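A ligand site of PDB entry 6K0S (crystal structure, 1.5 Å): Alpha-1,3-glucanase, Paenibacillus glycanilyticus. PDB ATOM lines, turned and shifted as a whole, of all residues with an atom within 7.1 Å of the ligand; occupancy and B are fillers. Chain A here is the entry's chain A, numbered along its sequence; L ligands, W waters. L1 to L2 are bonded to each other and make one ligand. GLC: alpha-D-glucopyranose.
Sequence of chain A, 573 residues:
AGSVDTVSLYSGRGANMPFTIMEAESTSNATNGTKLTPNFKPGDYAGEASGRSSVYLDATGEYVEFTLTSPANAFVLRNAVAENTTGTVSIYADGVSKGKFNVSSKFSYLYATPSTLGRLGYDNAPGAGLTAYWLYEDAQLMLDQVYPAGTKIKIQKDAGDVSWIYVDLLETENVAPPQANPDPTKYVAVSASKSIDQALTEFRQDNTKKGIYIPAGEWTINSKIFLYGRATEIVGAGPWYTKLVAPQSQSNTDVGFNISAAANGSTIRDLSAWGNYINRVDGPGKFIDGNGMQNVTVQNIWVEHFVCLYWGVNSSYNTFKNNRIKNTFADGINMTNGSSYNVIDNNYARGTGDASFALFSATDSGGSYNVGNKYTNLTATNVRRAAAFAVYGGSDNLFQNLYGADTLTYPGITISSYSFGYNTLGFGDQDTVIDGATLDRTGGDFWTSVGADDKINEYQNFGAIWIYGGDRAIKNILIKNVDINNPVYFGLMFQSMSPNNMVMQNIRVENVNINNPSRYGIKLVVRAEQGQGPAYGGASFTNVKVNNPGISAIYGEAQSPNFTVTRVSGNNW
An oxygen (O5) of GLC L2 sits close to the indole nitrogen (NE1) of Trp 311 (3.4 Å).
NH2 of Arg 280 is in hydrogen-bond range of O5 of GLC L1 (3.0 Å).
NZ of Lys 286 is in hydrogen-bond range of O4 of GLC L1, at 2.9 Å.
OD1 of Asp 282 is in hydrogen-bond range of O6 of GLC L1 (2.7 Å).
Water W12 lies within hydrogen-bond range of O6 of GLC L1 (2.8 Å), O of Pro 284 (2.8 Å), N of Gly 283 (2.8 Å), NZ of Lys 286 (3.0 Å) and O of Val 281 (3.2 Å).
Water W11 bridges an oxygen (O4) of GLC L2 (2.8 Å) and the side-chain hydroxyl (OH) of Tyr 422 (3.0 Å).
Water W1 lies within hydrogen-bond range of an oxygen (O2) of GLC L1 and the side-chain hydroxyl (OH) of Tyr 422.
Water W4 bridges an oxygen (O2) of GLC L2 (2.9 Å) and the backbone NH of Gly 283 (3.5 Å).
Water W2 lies within hydrogen-bond range of OD1 of Asp 331 (2.8 Å), NH2 of Arg 280 (3.1 Å), O1 of GLC L1 (3.3 Å) and OD2 of Asp 354 (3.3 Å).
Water W7 bridges OD1 of Asn 337 and O6 of GLC L2.
The side-chain carboxylate of Asp 354 lies within salt-bridge range of the guanidinium group of Arg 280, 2.8 Å away.
O of Gly 283 sits at hydrogen-bond distance from NZ of Lys 286, at 2.9 Å.
OD2 of Asp 282 sits at hydrogen-bond distance from OH of Tyr 122, at 2.6 Å.
OD1 of Asp 282 lies within salt-bridge range of NE of Arg 280.
The backbone carbonyl oxygen (O) of Ala 330 is in hydrogen-bond range of the backbone NH (N) of Asp 354.
The backbone NH (N) of Ala 330 is in hydrogen-bond range of the backbone carbonyl oxygen (O) of Val 307.
NE of Arg 280 is in hydrogen-bond range of OH of Tyr 122 (3.1 Å).
Val 281 touches the ligand.
Val 307 touches the ligand.
Ala 330 touches the ligand.
Tyr 422 touches the ligand.
Hydrophobic or aromatic side chains that line the ligand: Val 307, Trp 311, Ala 330 and Tyr 422.
Of the 21 residues printed, 8 come within 4 Å of the ligand.
Along chain A the residues within 4 Å of the ligand span positions 280 to 422.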
ATOM      1  N   TYR A 122     -14.146  24.422   6.593  1.00  0.00           N
ATOM      2  CA  TYR A 122     -14.032  23.119   7.270  1.00  0.00           C
ATOM      3  C   TYR A 122     -14.727  23.077   8.625  1.00  0.00           C
ATOM      4  O   TYR A 122     -15.128  21.992   9.061  1.00  0.00           O
ATOM      5  CB  TYR A 122     -12.557  22.752   7.487  1.00  0.00           C
ATOM      6  CG  TYR A 122     -11.818  22.287   6.252  1.00  0.00           C
ATOM      7  CD1 TYR A 122     -11.882  20.951   5.842  1.00  0.00           C
ATOM      8  CD2 TYR A 122     -11.022  23.158   5.520  1.00  0.00           C
ATOM      9  CE1 TYR A 122     -11.192  20.515   4.715  1.00  0.00           C
ATOM     10  CE2 TYR A 122     -10.326  22.728   4.399  1.00  0.00           C
ATOM     11  CZ  TYR A 122     -10.408  21.402   3.997  1.00  0.00           C
ATOM     12  OH  TYR A 122      -9.711  20.974   2.889  1.00  0.00           O
ATOM     13  N   ARG A 280     -17.063  21.560   4.860  1.00  0.00           N
ATOM     14  CA  ARG A 280     -16.282  20.798   3.909  1.00  0.00           C
ATOM     15  C   ARG A 280     -15.771  19.513   4.539  1.00  0.00           C
ATOM     16  O   ARG A 280     -15.317  19.503   5.696  1.00  0.00           O
ATOM     17  CB  ARG A 280     -15.118  21.645   3.409  1.00  0.00           C
ATOM     18  CG  ARG A 280     -14.187  20.949   2.430  1.00  0.00           C
ATOM     19  CD  ARG A 280     -13.163  21.952   1.918  1.00  0.00           C
ATOM     20  NE  ARG A 280     -12.204  21.331   1.010  1.00  0.00           N
ATOM     21  CZ  ARG A 280     -11.441  22.002   0.137  1.00  0.00           C
ATOM     22  NH1 ARG A 280     -11.527  23.327   0.060  1.00  0.00           N
ATOM     23  NH2 ARG A 280     -10.608  21.345  -0.657  1.00  0.00           N
ATOM     24  N   VAL A 281     -15.820  18.427   3.766  1.00  0.00           N
ATOM     25  CA  VAL A 281     -15.199  17.149   4.093  1.00  0.00           C
ATOM     26  C   VAL A 281     -14.475  16.683   2.837  1.00  0.00           C
ATOM     27  O   VAL A 281     -15.048  16.717   1.740  1.00  0.00           O
ATOM     28  CB  VAL A 281     -16.227  16.096   4.556  1.00  0.00           C
ATOM     29  CG1 VAL A 281     -15.537  14.796   5.003  1.00  0.00           C
ATOM     30  CG2 VAL A 281     -17.096  16.650   5.683  1.00  0.00           C
ATOM     31  N   ASP A 282     -13.222  16.269   2.972  1.00  0.00           N
ATOM     32  CA  ASP A 282     -12.406  15.903   1.819  1.00  0.00           C
ATOM     33  C   ASP A 282     -12.449  14.386   1.626  1.00  0.00           C
ATOM     34  O   ASP A 282     -11.981  13.628   2.493  1.00  0.00           O
ATOM     35  CB  ASP A 282     -10.967  16.383   1.988  1.00  0.00           C
ATOM     36  CG  ASP A 282     -10.853  17.887   1.958  1.00  0.00           C
ATOM     37  OD1 ASP A 282     -11.729  18.544   1.349  1.00  0.00           O
ATOM     38  OD2 ASP A 282      -9.883  18.427   2.522  1.00  0.00           O
ATOM     39  N   GLY A 283     -12.997  13.957   0.491  1.00  0.00           N
ATOM     40  CA  GLY A 283     -13.203  12.567   0.179  1.00  0.00           C
ATOM     41  C   GLY A 283     -14.616  12.365  -0.322  1.00  0.00           C
ATOM     42  O   GLY A 283     -14.877  12.383  -1.524  1.00  0.00           O
ATOM     43  N   PRO A 284     -15.558  12.202   0.605  1.00  0.00           N
ATOM     44  CA  PRO A 284     -16.968  12.155   0.235  1.00  0.00           C
ATOM     45  C   PRO A 284     -17.478  13.544  -0.131  1.00  0.00           C
ATOM     46  O   PRO A 284     -16.803  14.560   0.043  1.00  0.00           O
ATOM     47  CB  PRO A 284     -17.655  11.643   1.505  1.00  0.00           C
ATOM     48  CG  PRO A 284     -16.790  12.193   2.599  1.00  0.00           C
ATOM     49  CD  PRO A 284     -15.369  12.126   2.070  1.00  0.00           C
ATOM     50  N   LYS A 286     -19.272  14.614  -3.208  1.00  0.00           N
ATOM     51  CA  LYS A 286     -19.568  15.031  -4.562  1.00  0.00           C
ATOM     52  C   LYS A 286     -20.953  14.522  -4.934  1.00  0.00           C
ATOM     53  O   LYS A 286     -21.272  13.350  -4.701  1.00  0.00           O
ATOM     54  CB  LYS A 286     -18.519  14.512  -5.549  1.00  0.00           C
ATOM     55  CG  LYS A 286     -17.144  15.157  -5.373  1.00  0.00           C
ATOM     56  CD  LYS A 286     -16.233  14.340  -4.458  1.00  0.00           C
ATOM     57  CE  LYS A 286     -14.812  14.906  -4.476  1.00  0.00           C
ATOM     58  NZ  LYS A 286     -13.859  14.128  -3.631  1.00  0.00           N
ATOM     59  N   ASN A 291     -15.820   8.142 -11.605  1.00  0.00           N
ATOM     60  CA  ASN A 291     -14.398   8.148 -11.908  1.00  0.00           C
ATOM     61  C   ASN A 291     -14.143   7.453 -13.245  1.00  0.00           C
ATOM     62  O   ASN A 291     -14.616   6.340 -13.482  1.00  0.00           O
ATOM     63  CB  ASN A 291     -13.610   7.505 -10.772  1.00  0.00           C
ATOM     64  CG  ASN A 291     -13.194   8.525  -9.703  1.00  0.00           C
ATOM     65  OD1 ASN A 291     -13.873   9.534  -9.493  1.00  0.00           O
ATOM     66  ND2 ASN A 291     -12.069   8.284  -9.050  1.00  0.00           N
ATOM     67  N   VAL A 307     -20.146  19.053  -1.242  1.00  0.00           N
ATOM     68  CA  VAL A 307     -18.757  19.510  -1.325  1.00  0.00           C
ATOM     69  C   VAL A 307     -18.439  19.948  -2.750  1.00  0.00           C
ATOM     70  O   VAL A 307     -17.921  21.039  -2.969  1.00  0.00           O
ATOM     71  CB  VAL A 307     -17.804  18.425  -0.808  1.00  0.00           C
ATOM     72  CG1 VAL A 307     -16.365  18.919  -0.873  1.00  0.00           C
ATOM     73  CG2 VAL A 307     -18.167  18.055   0.625  1.00  0.00           C
ATOM     74  N   CYS A 308     -18.785  19.105  -3.742  1.00  0.00           N
ATOM     75  CA  CYS A 308     -18.650  19.488  -5.138  1.00  0.00           C
ATOM     76  C   CYS A 308     -19.854  18.995  -5.929  1.00  0.00           C
ATOM     77  O   CYS A 308     -20.594  18.107  -5.490  1.00  0.00           O
ATOM     78  CB  CYS A 308     -17.389  18.890  -5.802  1.00  0.00           C
ATOM     79  SG  CYS A 308     -15.884  19.012  -4.871  1.00  0.00           S
ATOM     80  N   TRP A 311     -16.054  15.864  -9.517  1.00  0.00           N
ATOM     81  CA  TRP A 311     -14.596  15.871  -9.441  1.00  0.00           C
ATOM     82  C   TRP A 311     -14.102  14.746 -10.347  1.00  0.00           C
ATOM     83  O   TRP A 311     -14.038  13.591  -9.929  1.00  0.00           O
ATOM     84  CB  TRP A 311     -14.119  15.673  -8.009  1.00  0.00           C
ATOM     85  CG  TRP A 311     -12.641  15.765  -7.813  1.00  0.00           C
ATOM     86  CD1 TRP A 311     -11.690  14.866  -8.224  1.00  0.00           C
ATOM     87  CD2 TRP A 311     -11.929  16.808  -7.128  1.00  0.00           C
ATOM     88  NE1 TRP A 311     -10.436  15.285  -7.837  1.00  0.00           N
ATOM     89  CE2 TRP A 311     -10.560  16.474  -7.164  1.00  0.00           C
ATOM     90  CE3 TRP A 311     -12.334  17.993  -6.488  1.00  0.00           C
ATOM     91  CZ2 TRP A 311      -9.587  17.290  -6.584  1.00  0.00           C
ATOM     92  CZ3 TRP A 311     -11.366  18.790  -5.919  1.00  0.00           C
ATOM     93  CH2 TRP A 311     -10.004  18.447  -5.974  1.00  0.00           C
ATOM     94  N   VAL A 313     -11.849  12.259 -12.648  1.00  0.00           N
ATOM     95  CA  VAL A 313     -10.543  11.592 -12.611  1.00  0.00           C
ATOM     96  C   VAL A 313     -10.462  10.753 -13.882  1.00  0.00           C
ATOM     97  O   VAL A 313     -11.133   9.729 -13.998  1.00  0.00           O
ATOM     98  CB  VAL A 313     -10.367  10.702 -11.371  1.00  0.00           C
ATOM     99  CG1 VAL A 313      -8.972  10.110 -11.365  1.00  0.00           C
ATOM    100  CG2 VAL A 313     -10.600  11.500 -10.098  1.00  0.00           C
ATOM    101  N   PHE A 329     -19.201  23.425  -0.593  1.00  0.00           N
ATOM    102  CA  PHE A 329     -18.161  23.562   0.416  1.00  0.00           C
ATOM    103  C   PHE A 329     -16.758  23.346  -0.128  1.00  0.00           C
ATOM    104  O   PHE A 329     -15.785  23.642   0.593  1.00  0.00           O
ATOM    105  CB  PHE A 329     -18.494  22.635   1.604  1.00  0.00           C
ATOM    106  CG  PHE A 329     -19.655  23.155   2.378  1.00  0.00           C
ATOM    107  CD1 PHE A 329     -19.454  24.121   3.365  1.00  0.00           C
ATOM    108  CD2 PHE A 329     -20.949  22.798   2.036  1.00  0.00           C
ATOM    109  CE1 PHE A 329     -20.541  24.654   4.049  1.00  0.00           C
ATOM    110  CE2 PHE A 329     -22.032  23.334   2.712  1.00  0.00           C
ATOM    111  CZ  PHE A 329     -21.818  24.272   3.716  1.00  0.00           C
ATOM    112  N   ALA A 330     -16.630  22.942  -1.386  1.00  0.00           N
ATOM    113  CA  ALA A 330     -15.375  23.024  -2.110  1.00  0.00           C
ATOM    114  C   ALA A 330     -15.658  23.288  -3.598  1.00  0.00           C
ATOM    115  O   ALA A 330     -16.599  24.025  -3.903  1.00  0.00           O
ATOM    116  CB  ALA A 330     -14.538  21.757  -1.925  1.00  0.00           C
ATOM    117  N   ASP A 331     -14.886  22.691  -4.504  1.00  0.00           N
ATOM    118  CA  ASP A 331     -14.927  23.049  -5.926  1.00  0.00           C
ATOM    119  C   ASP A 331     -16.312  22.842  -6.523  1.00  0.00           C
ATOM    120  O   ASP A 331     -17.068  21.981  -6.080  1.00  0.00           O
ATOM    121  CB  ASP A 331     -13.955  22.190  -6.765  1.00  0.00           C
ATOM    122  CG  ASP A 331     -12.518  22.284  -6.313  1.00  0.00           C
ATOM    123  OD1 ASP A 331     -12.241  22.168  -5.111  1.00  0.00           O
ATOM    124  OD2 ASP A 331     -11.646  22.391  -7.216  1.00  0.00           O
ATOM    125  N   ASN A 334     -14.337  20.136 -11.029  1.00  0.00           N
ATOM    126  CA  ASN A 334     -12.913  19.992 -11.242  1.00  0.00           C
ATOM    127  C   ASN A 334     -12.705  18.762 -12.119  1.00  0.00           C
ATOM    128  O   ASN A 334     -13.349  17.729 -11.889  1.00  0.00           O
ATOM    129  CB  ASN A 334     -12.171  19.829  -9.902  1.00  0.00           C
ATOM    130  CG  ASN A 334     -10.656  19.911 -10.041  1.00  0.00           C
ATOM    131  OD1 ASN A 334     -10.123  20.205 -11.112  1.00  0.00           O
ATOM    132  ND2 ASN A 334      -9.965  19.638  -8.944  1.00  0.00           N
ATOM    133  N   THR A 336      -9.697  16.273 -13.471  1.00  0.00           N
ATOM    134  CA  THR A 336      -8.306  16.000 -13.108  1.00  0.00           C
ATOM    135  C   THR A 336      -7.783  14.759 -13.824  1.00  0.00           C
ATOM    136  O   THR A 336      -8.538  13.979 -14.413  1.00  0.00           O
ATOM    137  CB  THR A 336      -8.128  15.815 -11.601  1.00  0.00           C
ATOM    138  OG1 THR A 336      -8.451  14.461 -11.235  1.00  0.00           O
ATOM    139  CG2 THR A 336      -9.012  16.778 -10.804  1.00  0.00           C
ATOM    140  N   ASN A 337      -6.453  14.619 -13.781  1.00  0.00           N
ATOM    141  CA  ASN A 337      -5.771  13.342 -13.988  1.00  0.00           C
ATOM    142  C   ASN A 337      -6.160  12.664 -15.300  1.00  0.00           C
ATOM    143  O   ASN A 337      -6.584  11.512 -15.326  1.00  0.00           O
ATOM    144  CB  ASN A 337      -6.032  12.402 -12.806  1.00  0.00           C
ATOM    145  CG  ASN A 337      -5.520  12.949 -11.492  1.00  0.00           C
ATOM    146  OD1 ASN A 337      -5.110  14.104 -11.400  1.00  0.00           O
ATOM    147  ND2 ASN A 337      -5.534  12.109 -10.456  1.00  0.00           N
ATOM    148  N   ASP A 354     -14.418  26.333  -2.902  1.00  0.00           N
ATOM    149  CA  ASP A 354     -13.076  26.254  -3.463  1.00  0.00           C
ATOM    150  C   ASP A 354     -13.260  26.607  -4.934  1.00  0.00           C
ATOM    151  O   ASP A 354     -14.324  27.127  -5.325  1.00  0.00           O
ATOM    152  CB  ASP A 354     -12.438  24.890  -3.202  1.00  0.00           C
ATOM    153  CG  ASP A 354     -10.902  24.917  -3.175  1.00  0.00           C
ATOM    154  OD1 ASP A 354     -10.286  25.343  -4.170  1.00  0.00           O
ATOM    155  OD2 ASP A 354     -10.315  24.490  -2.162  1.00  0.00           O
ATOM    156  N   PHE A 360      -7.174  20.280 -13.345  1.00  0.00           N
ATOM    157  CA  PHE A 360      -5.869  19.902 -12.795  1.00  0.00           C
ATOM    158  C   PHE A 360      -5.291  18.781 -13.646  1.00  0.00           C
ATOM    159  O   PHE A 360      -5.773  17.646 -13.597  1.00  0.00           O
ATOM    160  CB  PHE A 360      -5.960  19.483 -11.333  1.00  0.00           C
ATOM    161  CG  PHE A 360      -4.613  19.297 -10.678  1.00  0.00           C
ATOM    162  CD1 PHE A 360      -3.899  18.126 -10.871  1.00  0.00           C
ATOM    163  CD2 PHE A 360      -4.053  20.304  -9.904  1.00  0.00           C
ATOM    164  CE1 PHE A 360      -2.648  17.952 -10.293  1.00  0.00           C
ATOM    165  CE2 PHE A 360      -2.809  20.137  -9.327  1.00  0.00           C
ATOM    166  CZ  PHE A 360      -2.106  18.968  -9.512  1.00  0.00           C
ATOM    167  N   TYR A 422       1.984  15.952  -6.899  1.00  0.00           N
ATOM    168  CA  TYR A 422       1.462  14.920  -7.773  1.00  0.00           C
ATOM    169  C   TYR A 422       2.363  14.766  -8.995  1.00  0.00           C
ATOM    170  O   TYR A 422       3.268  15.563  -9.248  1.00  0.00           O
ATOM    171  CB  TYR A 422       0.029  15.234  -8.174  1.00  0.00           C
ATOM    172  CG  TYR A 422      -0.928  15.357  -7.007  1.00  0.00           C
ATOM    173  CD1 TYR A 422      -1.316  14.230  -6.283  1.00  0.00           C
ATOM    174  CD2 TYR A 422      -1.429  16.585  -6.623  1.00  0.00           C
ATOM    175  CE1 TYR A 422      -2.182  14.339  -5.210  1.00  0.00           C
ATOM    176  CE2 TYR A 422      -2.310  16.708  -5.551  1.00  0.00           C
ATOM    177  CZ  TYR A 422      -2.683  15.582  -4.844  1.00  0.00           C
ATOM    178  OH  TYR A 422      -3.550  15.691  -3.770  1.00  0.00           O
HETATM  179  C1  GLC L   1      -8.955  18.156  -1.549  1.00  0.00           C
HETATM  180  C2  GLC L   1      -8.786  16.680  -1.823  1.00  0.00           C
HETATM  181  C3  GLC L   1      -9.685  16.264  -2.957  1.00  0.00           C
HETATM  182  C4  GLC L   1     -11.124  16.627  -2.666  1.00  0.00           C
HETATM  183  C5  GLC L   1     -11.174  18.107  -2.464  1.00  0.00           C
HETATM  184  C6  GLC L   1     -12.580  18.524  -2.084  1.00  0.00           C
HETATM  185  O1  GLC L   1      -8.388  18.844  -2.620  1.00  0.00           O
HETATM  186  O2  GLC L   1      -7.423  16.409  -2.122  1.00  0.00           O
HETATM  187  O3  GLC L   1      -9.686  14.884  -3.020  1.00  0.00           O
HETATM  188  O4  GLC L   1     -11.962  16.264  -3.723  1.00  0.00           O
HETATM  189  O5  GLC L   1     -10.330  18.433  -1.408  1.00  0.00           O
HETATM  190  O6  GLC L   1     -13.000  17.907  -0.933  1.00  0.00           O
HETATM  191  C1  GLC L   2      -9.534  14.328  -4.370  1.00  0.00           C
HETATM  192  C2  GLC L   2      -9.752  12.815  -4.371  1.00  0.00           C
HETATM  193  C3  GLC L   2      -8.482  12.142  -3.838  1.00  0.00           C
HETATM  194  C4  GLC L   2      -7.265  12.595  -4.645  1.00  0.00           C
HETATM  195  C5  GLC L   2      -7.211  14.121  -4.707  1.00  0.00           C
HETATM  196  C6  GLC L   2      -6.052  14.625  -5.566  1.00  0.00           C
HETATM  197  O2  GLC L   2     -10.878  12.514  -3.572  1.00  0.00           O
HETATM  198  O3  GLC L   2      -8.610  10.735  -3.868  1.00  0.00           O
HETATM  199  O4  GLC L   2      -6.084  12.106  -4.062  1.00  0.00           O
HETATM  200  O5  GLC L   2      -8.437  14.626  -5.208  1.00  0.00           O
HETATM  201  O6  GLC L   2      -6.140  14.154  -6.890  1.00  0.00           O
HETATM  202  O   HOH W   1      -5.938  17.869  -4.065  1.00  0.00           O
HETATM  203  O   HOH W   2      -9.917  21.572  -3.626  1.00  0.00           O
HETATM  204  O   HOH W   3     -13.779  11.657  -5.101  1.00  0.00           O
HETATM  205  O   HOH W   4     -10.067  12.540  -0.757  1.00  0.00           O
HETATM  206  O   HOH W   5      -5.929  16.676  -8.544  1.00  0.00           O
HETATM  207  O   HOH W   6      -8.040  13.845  -8.495  1.00  0.00           O
HETATM  208  O   HOH W   7      -4.083  15.247  -9.410  1.00  0.00           O
HETATM  209  O   HOH W   8      -4.153  11.259  -6.440  1.00  0.00           O
HETATM  210  O   HOH W   9     -11.956  10.177  -4.078  1.00  0.00           O
HETATM  211  O   HOH W  10      -9.451   9.932  -1.266  1.00  0.00           O
HETATM  212  O   HOH W  11      -4.775  13.555  -2.012  1.00  0.00           O
HETATM  213  O   HOH W  12     -14.537  15.631  -1.182  1.00  0.00           O
HETATM  214  O   HOH W  13      -6.807  20.904  -1.472  1.00  0.00           O
